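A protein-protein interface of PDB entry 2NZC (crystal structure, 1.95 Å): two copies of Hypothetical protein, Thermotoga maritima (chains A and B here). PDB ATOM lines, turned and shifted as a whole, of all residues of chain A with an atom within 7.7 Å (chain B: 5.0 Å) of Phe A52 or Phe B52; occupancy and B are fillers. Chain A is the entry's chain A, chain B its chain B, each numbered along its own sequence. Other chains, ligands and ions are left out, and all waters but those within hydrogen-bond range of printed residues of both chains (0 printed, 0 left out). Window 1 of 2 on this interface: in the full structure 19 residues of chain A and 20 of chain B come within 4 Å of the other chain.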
ATOM      1  N   TYR A   8       8.888  15.910  -7.020  1.00  0.00           N
ATOM      2  CA  TYR A   8       9.291  15.609  -5.655  1.00  0.00           C
ATOM      3  C   TYR A   8       8.471  14.490  -5.104  1.00  0.00           C
ATOM      4  O   TYR A   8       7.284  14.328  -5.430  1.00  0.00           O
ATOM      5  CB  TYR A   8       9.097  16.792  -4.701  1.00  0.00           C
ATOM      6  CG  TYR A   8       9.893  17.982  -5.074  1.00  0.00           C
ATOM      7  CD1 TYR A   8      11.200  18.130  -4.630  1.00  0.00           C
ATOM      8  CD2 TYR A   8       9.338  18.991  -5.872  1.00  0.00           C
ATOM      9  CE1 TYR A   8      11.944  19.234  -4.981  1.00  0.00           C
ATOM     10  CE2 TYR A   8      10.072  20.086  -6.236  1.00  0.00           C
ATOM     11  CZ  TYR A   8      11.373  20.214  -5.785  1.00  0.00           C
ATOM     12  OH  TYR A   8      12.122  21.307  -6.156  1.00  0.00           O
ATOM     13  N   ILE A   9       9.104  13.708  -4.249  1.00  0.00           N
ATOM     14  CA  ILE A   9       8.407  12.616  -3.613  1.00  0.00           C
ATOM     15  C   ILE A   9       8.353  12.942  -2.129  1.00  0.00           C
ATOM     16  O   ILE A   9       9.360  13.355  -1.563  1.00  0.00           O
ATOM     17  CB  ILE A   9       9.159  11.317  -3.849  1.00  0.00           C
ATOM     18  CG1 ILE A   9       9.338  11.084  -5.351  1.00  0.00           C
ATOM     19  CG2 ILE A   9       8.453  10.178  -3.169  1.00  0.00           C
ATOM     20  CD1 ILE A   9      10.513  10.183  -5.678  1.00  0.00           C
ATOM     21  N   LEU A  10       7.196  12.774  -1.507  1.00  0.00           N
ATOM     22  CA  LEU A  10       7.097  12.978  -0.055  1.00  0.00           C
ATOM     23  C   LEU A  10       6.645  11.686   0.547  1.00  0.00           C
ATOM     24  O   LEU A  10       5.696  11.066   0.072  1.00  0.00           O
ATOM     25  CB  LEU A  10       6.072  14.044   0.323  1.00  0.00           C
ATOM     26  CG  LEU A  10       6.542  15.490   0.435  1.00  0.00           C
ATOM     27  CD1 LEU A  10       6.936  15.971  -0.918  1.00  0.00           C
ATOM     28  CD2 LEU A  10       5.486  16.377   1.019  1.00  0.00           C
ATOM     29  N   THR A  11       7.334  11.273   1.597  1.00  0.00           N
ATOM     30  CA  THR A  11       6.867  10.168   2.408  1.00  0.00           C
ATOM     31  C   THR A  11       6.489  10.753   3.769  1.00  0.00           C
ATOM     32  O   THR A  11       7.291  11.468   4.381  1.00  0.00           O
ATOM     33  CB  THR A  11       7.961   9.146   2.595  1.00  0.00           C
ATOM     34  OG1 THR A  11       8.356   8.641   1.302  1.00  0.00           O
ATOM     35  CG2 THR A  11       7.455   7.986   3.465  1.00  0.00           C
ATOM     36  N   ILE A  12       5.299  10.417   4.237  1.00  0.00           N
ATOM     37  CA  ILE A  12       4.767  10.900   5.505  1.00  0.00           C
ATOM     38  C   ILE A  12       4.403   9.718   6.391  1.00  0.00           C
ATOM     39  O   ILE A  12       3.734   8.785   5.941  1.00  0.00           O
ATOM     40  CB  ILE A  12       3.554  11.758   5.255  1.00  0.00           C
ATOM     41  CG1 ILE A  12       3.941  12.977   4.386  1.00  0.00           C
ATOM     42  CG2 ILE A  12       2.915  12.253   6.606  1.00  0.00           C
ATOM     43  CD1 ILE A  12       2.748  13.730   3.853  1.00  0.00           C
ATOM     44  N   VAL A  13       4.853   9.745   7.642  1.00  0.00           N
ATOM     45  CA  VAL A  13       4.426   8.759   8.634  1.00  0.00           C
ATOM     46  C   VAL A  13       3.692   9.532   9.730  1.00  0.00           C
ATOM     47  O   VAL A  13       4.222  10.521  10.242  1.00  0.00           O
ATOM     48  CB  VAL A  13       5.611   7.968   9.229  1.00  0.00           C
ATOM     49  CG1 VAL A  13       5.132   7.050  10.339  1.00  0.00           C
ATOM     50  CG2 VAL A  13       6.299   7.148   8.127  1.00  0.00           C
ATOM     51  N   LEU A  28      -2.565  19.193   3.068  1.00  0.00           N
ATOM     52  CA  LEU A  28      -2.487  18.611   1.732  1.00  0.00           C
ATOM     53  C   LEU A  28      -3.635  19.102   0.845  1.00  0.00           C
ATOM     54  O   LEU A  28      -3.473  19.280  -0.367  1.00  0.00           O
ATOM     55  CB  LEU A  28      -2.436  17.084   1.791  1.00  0.00           C
ATOM     56  CG  LEU A  28      -1.252  16.432   2.539  1.00  0.00           C
ATOM     57  CD1 LEU A  28      -1.428  14.895   2.575  1.00  0.00           C
ATOM     58  CD2 LEU A  28       0.123  16.841   1.937  1.00  0.00           C
ATOM     59  N   ILE A  35      -0.411  17.874  -6.515  1.00  0.00           N
ATOM     60  CA  ILE A  35      -0.261  16.470  -6.138  1.00  0.00           C
ATOM     61  C   ILE A  35      -0.660  15.643  -7.330  1.00  0.00           C
ATOM     62  O   ILE A  35      -1.760  15.829  -7.869  1.00  0.00           O
ATOM     63  CB  ILE A  35      -1.160  16.105  -4.933  1.00  0.00           C
ATOM     64  CG1 ILE A  35      -0.645  16.798  -3.679  1.00  0.00           C
ATOM     65  CG2 ILE A  35      -1.234  14.542  -4.728  1.00  0.00           C
ATOM     66  CD1 ILE A  35      -1.557  16.608  -2.469  1.00  0.00           C
ATOM     67  N   LEU A  37      -0.148  12.153  -7.222  1.00  0.00           N
ATOM     68  CA  LEU A  37      -0.441  10.767  -6.785  1.00  0.00           C
ATOM     69  C   LEU A  37      -0.467  10.782  -5.290  1.00  0.00           C
ATOM     70  O   LEU A  37       0.448  11.337  -4.674  1.00  0.00           O
ATOM     71  CB  LEU A  37       0.678   9.798  -7.205  1.00  0.00           C
ATOM     72  CG  LEU A  37       0.448   8.331  -6.783  1.00  0.00           C
ATOM     73  CD1 LEU A  37      -0.792   7.777  -7.497  1.00  0.00           C
ATOM     74  CD2 LEU A  37       1.658   7.466  -7.047  1.00  0.00           C
ATOM     75  N   ARG A  38      -1.469  10.149  -4.693  1.00  0.00           N
ATOM     76  CA  ARG A  38      -1.413  10.013  -3.228  1.00  0.00           C
ATOM     77  C   ARG A  38      -1.777   8.595  -2.866  1.00  0.00           C
ATOM     78  O   ARG A  38      -2.781   8.099  -3.327  1.00  0.00           O
ATOM     79  CB  ARG A  38      -2.399  10.981  -2.562  1.00  0.00           C
ATOM     80  CG  ARG A  38      -2.447  10.796  -0.983  1.00  0.00           C
ATOM     81  CD  ARG A  38      -3.284  11.960  -0.368  1.00  0.00           C
ATOM     82  NE  ARG A  38      -3.553  11.678   1.054  1.00  0.00           N
ATOM     83  CZ  ARG A  38      -4.152  12.512   1.903  1.00  0.00           C
ATOM     84  NH1 ARG A  38      -4.585  13.706   1.493  1.00  0.00           N
ATOM     85  NH2 ARG A  38      -4.357  12.114   3.159  1.00  0.00           N
ATOM     86  N   VAL A  39      -0.967   7.960  -2.026  1.00  0.00           N
ATOM     87  CA  VAL A  39      -1.207   6.557  -1.631  1.00  0.00           C
ATOM     88  C   VAL A  39      -1.240   6.554  -0.104  1.00  0.00           C
ATOM     89  O   VAL A  39      -0.276   7.014   0.532  1.00  0.00           O
ATOM     90  CB  VAL A  39      -0.070   5.634  -2.113  1.00  0.00           C
ATOM     91  CG1 VAL A  39      -0.345   4.168  -1.641  1.00  0.00           C
ATOM     92  CG2 VAL A  39      -0.010   5.687  -3.647  1.00  0.00           C
ATOM     93  N   GLY A  40      -2.325   6.082   0.478  1.00  0.00           N
ATOM     94  CA  GLY A  40      -2.417   5.984   1.931  1.00  0.00           C
ATOM     95  C   GLY A  40      -2.517   4.527   2.343  1.00  0.00           C
ATOM     96  O   GLY A  40      -3.320   3.778   1.790  1.00  0.00           O
ATOM     97  N   TYR A  41      -1.697   4.125   3.322  1.00  0.00           N
ATOM     98  CA  TYR A  41      -1.611   2.732   3.764  1.00  0.00           C
ATOM     99  C   TYR A  41      -1.600   2.758   5.274  1.00  0.00           C
ATOM    100  O   TYR A  41      -0.592   3.157   5.888  1.00  0.00           O
ATOM    101  CB  TYR A  41      -0.336   2.077   3.217  1.00  0.00           C
ATOM    102  CG  TYR A  41      -0.096   0.654   3.717  1.00  0.00           C
ATOM    103  CD1 TYR A  41      -0.738  -0.432   3.118  1.00  0.00           C
ATOM    104  CD2 TYR A  41       0.748   0.389   4.806  1.00  0.00           C
ATOM    105  CE1 TYR A  41      -0.515  -1.698   3.538  1.00  0.00           C
ATOM    106  CE2 TYR A  41       0.945  -0.923   5.275  1.00  0.00           C
ATOM    107  CZ  TYR A  41       0.319  -1.950   4.622  1.00  0.00           C
ATOM    108  OH  TYR A  41       0.493  -3.241   5.023  1.00  0.00           O
ATOM    109  N   ALA A  49      -0.199   5.562  10.151  1.00  0.00           N
ATOM    110  CA  ALA A  49      -0.552   5.481   8.733  1.00  0.00           C
ATOM    111  C   ALA A  49       0.614   6.022   7.936  1.00  0.00           C
ATOM    112  O   ALA A  49       1.346   6.880   8.419  1.00  0.00           O
ATOM    113  CB  ALA A  49      -1.792   6.295   8.450  1.00  0.00           C
ATOM    114  N   ILE A  50       0.768   5.529   6.706  1.00  0.00           N
ATOM    115  CA  ILE A  50       1.831   5.960   5.787  1.00  0.00           C
ATOM    116  C   ILE A  50       1.152   6.677   4.647  1.00  0.00           C
ATOM    117  O   ILE A  50       0.136   6.207   4.158  1.00  0.00           O
ATOM    118  CB  ILE A  50       2.609   4.716   5.221  1.00  0.00           C
ATOM    119  CG1 ILE A  50       3.365   4.019   6.348  1.00  0.00           C
ATOM    120  CG2 ILE A  50       3.575   5.131   4.081  1.00  0.00           C
ATOM    121  CD1 ILE A  50       3.834   2.554   6.004  1.00  0.00           C
ATOM    122  N   ILE A  51       1.697   7.815   4.230  1.00  0.00           N
ATOM    123  CA  ILE A  51       1.234   8.490   3.033  1.00  0.00           C
ATOM    124  C   ILE A  51       2.416   8.686   2.102  1.00  0.00           C
ATOM    125  O   ILE A  51       3.478   9.221   2.527  1.00  0.00           O
ATOM    126  CB  ILE A  51       0.638   9.887   3.355  1.00  0.00           C
ATOM    127  CG1 ILE A  51      -0.482   9.775   4.381  1.00  0.00           C
ATOM    128  CG2 ILE A  51       0.100  10.583   2.071  1.00  0.00           C
ATOM    129  CD1 ILE A  51      -0.928  11.143   4.950  1.00  0.00           C
ATOM    130  N   PHE A  52       2.232   8.287   0.831  1.00  0.00           N
ATOM    131  CA  PHE A  52       3.244   8.540  -0.210  1.00  0.00           C
ATOM    132  C   PHE A  52       2.634   9.548  -1.172  1.00  0.00           C
ATOM    133  O   PHE A  52       1.473   9.399  -1.569  1.00  0.00           O
ATOM    134  CB  PHE A  52       3.537   7.314  -1.047  1.00  0.00           C
ATOM    135  CG  PHE A  52       4.165   6.166  -0.295  1.00  0.00           C
ATOM    136  CD1 PHE A  52       5.511   6.219   0.084  1.00  0.00           C
ATOM    137  CD2 PHE A  52       3.446   5.001  -0.062  1.00  0.00           C
ATOM    138  CE1 PHE A  52       6.136   5.106   0.720  1.00  0.00           C
ATOM    139  CE2 PHE A  52       4.055   3.898   0.576  1.00  0.00           C
ATOM    140  CZ  PHE A  52       5.388   3.956   0.972  1.00  0.00           C
ATOM    141  N   LEU A  53       3.411  10.537  -1.576  1.00  0.00           N
ATOM    142  CA  LEU A  53       2.910  11.564  -2.524  1.00  0.00           C
ATOM    143  C   LEU A  53       3.956  11.839  -3.574  1.00  0.00           C
ATOM    144  O   LEU A  53       5.167  11.878  -3.289  1.00  0.00           O
ATOM    145  CB  LEU A  53       2.613  12.910  -1.818  1.00  0.00           C
ATOM    146  CG  LEU A  53       1.706  12.972  -0.585  1.00  0.00           C
ATOM    147  CD1 LEU A  53       2.038  14.248   0.183  1.00  0.00           C
ATOM    148  CD2 LEU A  53       0.241  13.012  -0.993  1.00  0.00           C
ATOM    149  N   VAL A  54       3.485  12.086  -4.792  1.00  0.00           N
ATOM    150  CA  VAL A  54       4.323  12.646  -5.812  1.00  0.00           C
ATOM    151  C   VAL A  54       3.758  14.007  -6.179  1.00  0.00           C
ATOM    152  O   VAL A  54       2.548  14.126  -6.445  1.00  0.00           O
ATOM    153  CB  VAL A  54       4.351  11.712  -7.066  1.00  0.00           C
ATOM    154  CG1 VAL A  54       5.197  12.352  -8.174  1.00  0.00           C
ATOM    155  CG2 VAL A  54       4.906  10.343  -6.657  1.00  0.00           C
ATOM    156  N   LEU A  55       4.627  15.025  -6.226  1.00  0.00           N
ATOM    157  CA  LEU A  55       4.217  16.392  -6.544  1.00  0.00           C
ATOM    158  C   LEU A  55       5.026  16.894  -7.708  1.00  0.00           C
ATOM    159  O   LEU A  55       6.173  16.460  -7.904  1.00  0.00           O
ATOM    160  CB  LEU A  55       4.463  17.350  -5.364  1.00  0.00           C
ATOM    161  CG  LEU A  55       3.592  17.084  -4.149  1.00  0.00           C
ATOM    162  CD1 LEU A  55       4.300  16.188  -3.186  1.00  0.00           C
ATOM    163  CD2 LEU A  55       3.134  18.395  -3.468  1.00  0.00           C
ATOM    164  N   VAL A  80      12.172  13.791  -1.174  1.00  0.00           N
ATOM    165  CA  VAL A  80      13.222  13.331  -2.100  1.00  0.00           C
ATOM    166  C   VAL A  80      12.950  14.000  -3.440  1.00  0.00           C
ATOM    167  O   VAL A  80      11.913  13.702  -4.049  1.00  0.00           O
ATOM    168  CB  VAL A  80      13.099  11.789  -2.378  1.00  0.00           C
ATOM    169  CG1 VAL A  80      14.294  11.270  -3.225  1.00  0.00           C
ATOM    170  CG2 VAL A  80      12.943  10.980  -1.099  1.00  0.00           C
ATOM    171  N   ILE B   9       9.748   1.601   4.985  1.00  0.00           N
ATOM    172  CA  ILE B   9       9.228   2.234   3.806  1.00  0.00           C
ATOM    173  C   ILE B   9      10.437   2.438   2.904  1.00  0.00           C
ATOM    174  O   ILE B   9      11.449   2.939   3.380  1.00  0.00           O
ATOM    175  CB  ILE B   9       8.710   3.645   4.161  1.00  0.00           C
ATOM    176  CG1 ILE B   9       7.758   3.622   5.360  1.00  0.00           C
ATOM    177  CG2 ILE B   9       8.011   4.246   2.974  1.00  0.00           C
ATOM    178  CD1 ILE B   9       6.497   2.959   5.053  1.00  0.00           C
ATOM    179  N   LEU B  10      10.342   2.096   1.622  1.00  0.00           N
ATOM    180  CA  LEU B  10      11.434   2.427   0.687  1.00  0.00           C
ATOM    181  C   LEU B  10      10.904   3.297  -0.395  1.00  0.00           C
ATOM    182  O   LEU B  10       9.796   3.065  -0.885  1.00  0.00           O
ATOM    183  CB  LEU B  10      12.016   1.173   0.022  1.00  0.00           C
ATOM    184  CG  LEU B  10      13.115   0.517   0.834  1.00  0.00           C
ATOM    185  CD1 LEU B  10      12.463  -0.201   1.982  1.00  0.00           C
ATOM    186  CD2 LEU B  10      13.891  -0.471  -0.016  1.00  0.00           C
ATOM    187  N   THR B  11      11.693   4.289  -0.789  1.00  0.00           N
ATOM    188  CA  THR B  11      11.421   5.028  -2.006  1.00  0.00           C
ATOM    189  C   THR B  11      12.571   4.760  -2.946  1.00  0.00           C
ATOM    190  O   THR B  11      13.740   4.917  -2.574  1.00  0.00           O
ATOM    191  CB  THR B  11      11.339   6.536  -1.744  1.00  0.00           C
ATOM    192  OG1 THR B  11      10.285   6.803  -0.813  1.00  0.00           O
ATOM    193  CG2 THR B  11      11.032   7.266  -3.012  1.00  0.00           C
ATOM    194  N   LEU B  37       3.210  -3.843  -0.040  1.00  0.00           N
ATOM    195  CA  LEU B  37       2.617  -2.892  -0.965  1.00  0.00           C
ATOM    196  C   LEU B  37       3.712  -2.473  -1.930  1.00  0.00           C
ATOM    197  O   LEU B  37       4.839  -2.243  -1.510  1.00  0.00           O
ATOM    198  CB  LEU B  37       2.134  -1.650  -0.208  1.00  0.00           C
ATOM    199  CG  LEU B  37       1.548  -0.523  -1.050  1.00  0.00           C
ATOM    200  CD1 LEU B  37       0.303  -0.972  -1.790  1.00  0.00           C
ATOM    201  CD2 LEU B  37       1.301   0.724  -0.204  1.00  0.00           C
ATOM    202  N   ARG B  38       3.365  -2.364  -3.212  1.00  0.00           N
ATOM    203  CA  ARG B  38       4.338  -1.835  -4.179  1.00  0.00           C
ATOM    204  C   ARG B  38       3.574  -0.920  -5.099  1.00  0.00           C
ATOM    205  O   ARG B  38       2.572  -1.312  -5.663  1.00  0.00           O
ATOM    206  CB  ARG B  38       4.986  -2.964  -4.986  1.00  0.00           C
ATOM    207  CG  ARG B  38       5.889  -2.437  -6.122  1.00  0.00           C
ATOM    208  CD  ARG B  38       6.673  -3.564  -6.791  1.00  0.00           C
ATOM    209  NE  ARG B  38       7.435  -3.078  -7.943  1.00  0.00           N
ATOM    210  CZ  ARG B  38       8.312  -3.824  -8.616  1.00  0.00           C
ATOM    211  NH1 ARG B  38       8.530  -5.086  -8.254  1.00  0.00           N
ATOM    212  NH2 ARG B  38       8.942  -3.330  -9.669  1.00  0.00           N
ATOM    213  N   VAL B  39       4.062   0.297  -5.241  1.00  0.00           N
ATOM    214  CA  VAL B  39       3.444   1.256  -6.150  1.00  0.00           C
ATOM    215  C   VAL B  39       4.485   1.689  -7.174  1.00  0.00           C
ATOM    216  O   VAL B  39       5.595   2.089  -6.807  1.00  0.00           O
ATOM    217  CB  VAL B  39       2.964   2.463  -5.319  1.00  0.00           C
ATOM    218  CG1 VAL B  39       2.387   3.551  -6.203  1.00  0.00           C
ATOM    219  CG2 VAL B  39       1.924   2.010  -4.274  1.00  0.00           C
ATOM    220  N   ILE B  50       9.327   5.936 -10.377  1.00  0.00           N
ATOM    221  CA  ILE B  50       9.342   5.942  -8.920  1.00  0.00           C
ATOM    222  C   ILE B  50       8.730   4.621  -8.483  1.00  0.00           C
ATOM    223  O   ILE B  50       7.725   4.166  -9.053  1.00  0.00           O
ATOM    224  CB  ILE B  50       8.540   7.162  -8.340  1.00  0.00           C
ATOM    225  CG1 ILE B  50       9.242   8.458  -8.719  1.00  0.00           C
ATOM    226  CG2 ILE B  50       8.375   7.064  -6.808  1.00  0.00           C
ATOM    227  CD1 ILE B  50       8.331   9.713  -8.621  1.00  0.00           C
ATOM    228  N   ILE B  51       9.361   3.972  -7.507  1.00  0.00           N
ATOM    229  CA  ILE B  51       8.742   2.816  -6.841  1.00  0.00           C
ATOM    230  C   ILE B  51       8.660   3.086  -5.349  1.00  0.00           C
ATOM    231  O   ILE B  51       9.632   3.571  -4.748  1.00  0.00           O
ATOM    232  CB  ILE B  51       9.544   1.514  -7.049  1.00  0.00           C
ATOM    233  CG1 ILE B  51       9.827   1.267  -8.527  1.00  0.00           C
ATOM    234  CG2 ILE B  51       8.794   0.319  -6.400  1.00  0.00           C
ATOM    235  CD1 ILE B  51      10.917   0.257  -8.781  1.00  0.00           C
ATOM    236  N   PHE B  52       7.497   2.818  -4.754  1.00  0.00           N
ATOM    237  CA  PHE B  52       7.295   2.955  -3.311  1.00  0.00           C
ATOM    238  C   PHE B  52       7.070   1.555  -2.804  1.00  0.00           C
ATOM    239  O   PHE B  52       6.267   0.800  -3.388  1.00  0.00           O
ATOM    240  CB  PHE B  52       6.013   3.731  -2.964  1.00  0.00           C
ATOM    241  CG  PHE B  52       6.009   5.172  -3.403  1.00  0.00           C
ATOM    242  CD1 PHE B  52       6.894   6.091  -2.846  1.00  0.00           C
ATOM    243  CD2 PHE B  52       5.070   5.626  -4.314  1.00  0.00           C
ATOM    244  CE1 PHE B  52       6.846   7.445  -3.231  1.00  0.00           C
ATOM    245  CE2 PHE B  52       5.022   6.965  -4.687  1.00  0.00           C
ATOM    246  CZ  PHE B  52       5.927   7.867  -4.147  1.00  0.00           C
ATOM    247  N   LEU B  53       7.696   1.224  -1.684  1.00  0.00           N
ATOM    248  CA  LEU B  53       7.508  -0.114  -1.080  1.00  0.00           C
ATOM    249  C   LEU B  53       7.214   0.012   0.393  1.00  0.00           C
ATOM    250  O   LEU B  53       7.745   0.910   1.040  1.00  0.00           O
ATOM    251  CB  LEU B  53       8.784  -0.958  -1.248  1.00  0.00           C
ATOM    252  CG  LEU B  53       9.321  -1.307  -2.635  1.00  0.00           C
ATOM    253  CD1 LEU B  53      10.641  -2.121  -2.495  1.00  0.00           C
ATOM    254  CD2 LEU B  53       8.330  -2.181  -3.390  1.00  0.00           C
ATOM    255  N   VAL B  54       6.314  -0.826   0.899  1.00  0.00           N
ATOM    256  CA  VAL B  54       6.218  -1.091   2.336  1.00  0.00           C
ATOM    257  C   VAL B  54       6.553  -2.556   2.565  1.00  0.00           C
ATOM    258  O   VAL B  54       5.974  -3.424   1.898  1.00  0.00           O
ATOM    259  CB  VAL B  54       4.786  -0.788   2.888  1.00  0.00           C
ATOM    260  CG1 VAL B  54       4.745  -1.039   4.454  1.00  0.00           C
ATOM    261  CG2 VAL B  54       4.370   0.640   2.532  1.00  0.00           C
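Hydrophobic or aromatic side chains of chain A within 4 Å of the printed part of chain B: Ile A9, Tyr A41, Ile A50, Phe A52 and Val A54. Among the printed residues, 13 pairs touch across the chains.
Phe A52 touches just these residues of chain B: Ile B9 (3.1 Å), Phe B52 (3.2 Å), Leu B53 (3.9 Å) and Val B54 (3.8 Å). Printed residues of chain A within 4 Å of Thr B11: Ile A9 (3.9 Å) and Thr A11 (3.4 Å). Of the printed residues of chain A, Ile B50 touches Ile A9 and Val A54. Of the printed residues of chain B, Ile A50 touches Ile B9. Printed residues of chain B within 4 Å of Ile A9: Thr B11, Ile B50 and Phe B52. The nearest residue of chain B that does not touch Phe A52 is Leu B37 (4.3 Å). The nearest residue of chain A that does not touch Phe B52 is Leu A37 (4.1 Å).
N of Ile A9 is in hydrogen-bond range of O of Val A80. The backbone NH of Phe A52 sits at hydrogen-bond distance from the backbone carbonyl oxygen of Val A39, 2.8 Å away. The backbone carbonyl oxygen of Tyr A41 is in hydrogen-bond range of the backbone NH of Ile A50. O of Leu B10 sits at hydrogen-bond distance from N of Leu B53, at 2.9 Å. O of Leu B37 is in hydrogen-bond range of N of Val B54. The backbone NH (N) of Phe B52 lies within hydrogen-bond range of the backbone carbonyl oxygen (O) of Val B39 (2.9 Å).
Ile A9 touches Thr B11, and with the chains exchanged Thr A11 touches Ile B9. Ile A9 touches Phe B52, and with the chains exchanged Phe A52 touches Ile B9. Phe A52 touches Val B54, and with the chains exchanged Val A54 touches Phe B52. Val A54 touches Ile B50, but with the chains exchanged Ile A50 does not touch Val B54 (4.001 Å). 11 positions are printed for both chains.
Among the printed residues, merely in contact across the chains: Ile A9 with Thr B11 (3.9 Å), Ile A9 with Ile B50 (3.7 Å), Ile A9 with Phe B52 (3.2 Å), Thr A11 with Ile B9 (3.8 Å), Tyr A41 with Val B54 (3.9 Å), Ile A50 with Ile B9 (2.9 Å), Phe A52 with Ile B9 (3.1 Å), Phe A52 with Phe B52 (3.2 Å), Phe A52 with Leu B53 (3.9 Å), Phe A52 with Val B54 (3.8 Å), Val A54 with Ile B50 (3.998 Å) and Val A54 with Phe B52 (3.7 Å).
The side-chain hydroxyl of Thr A11 is in hydrogen-bond range of the side-chain hydroxyl of Thr B11 (3.4 Å).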
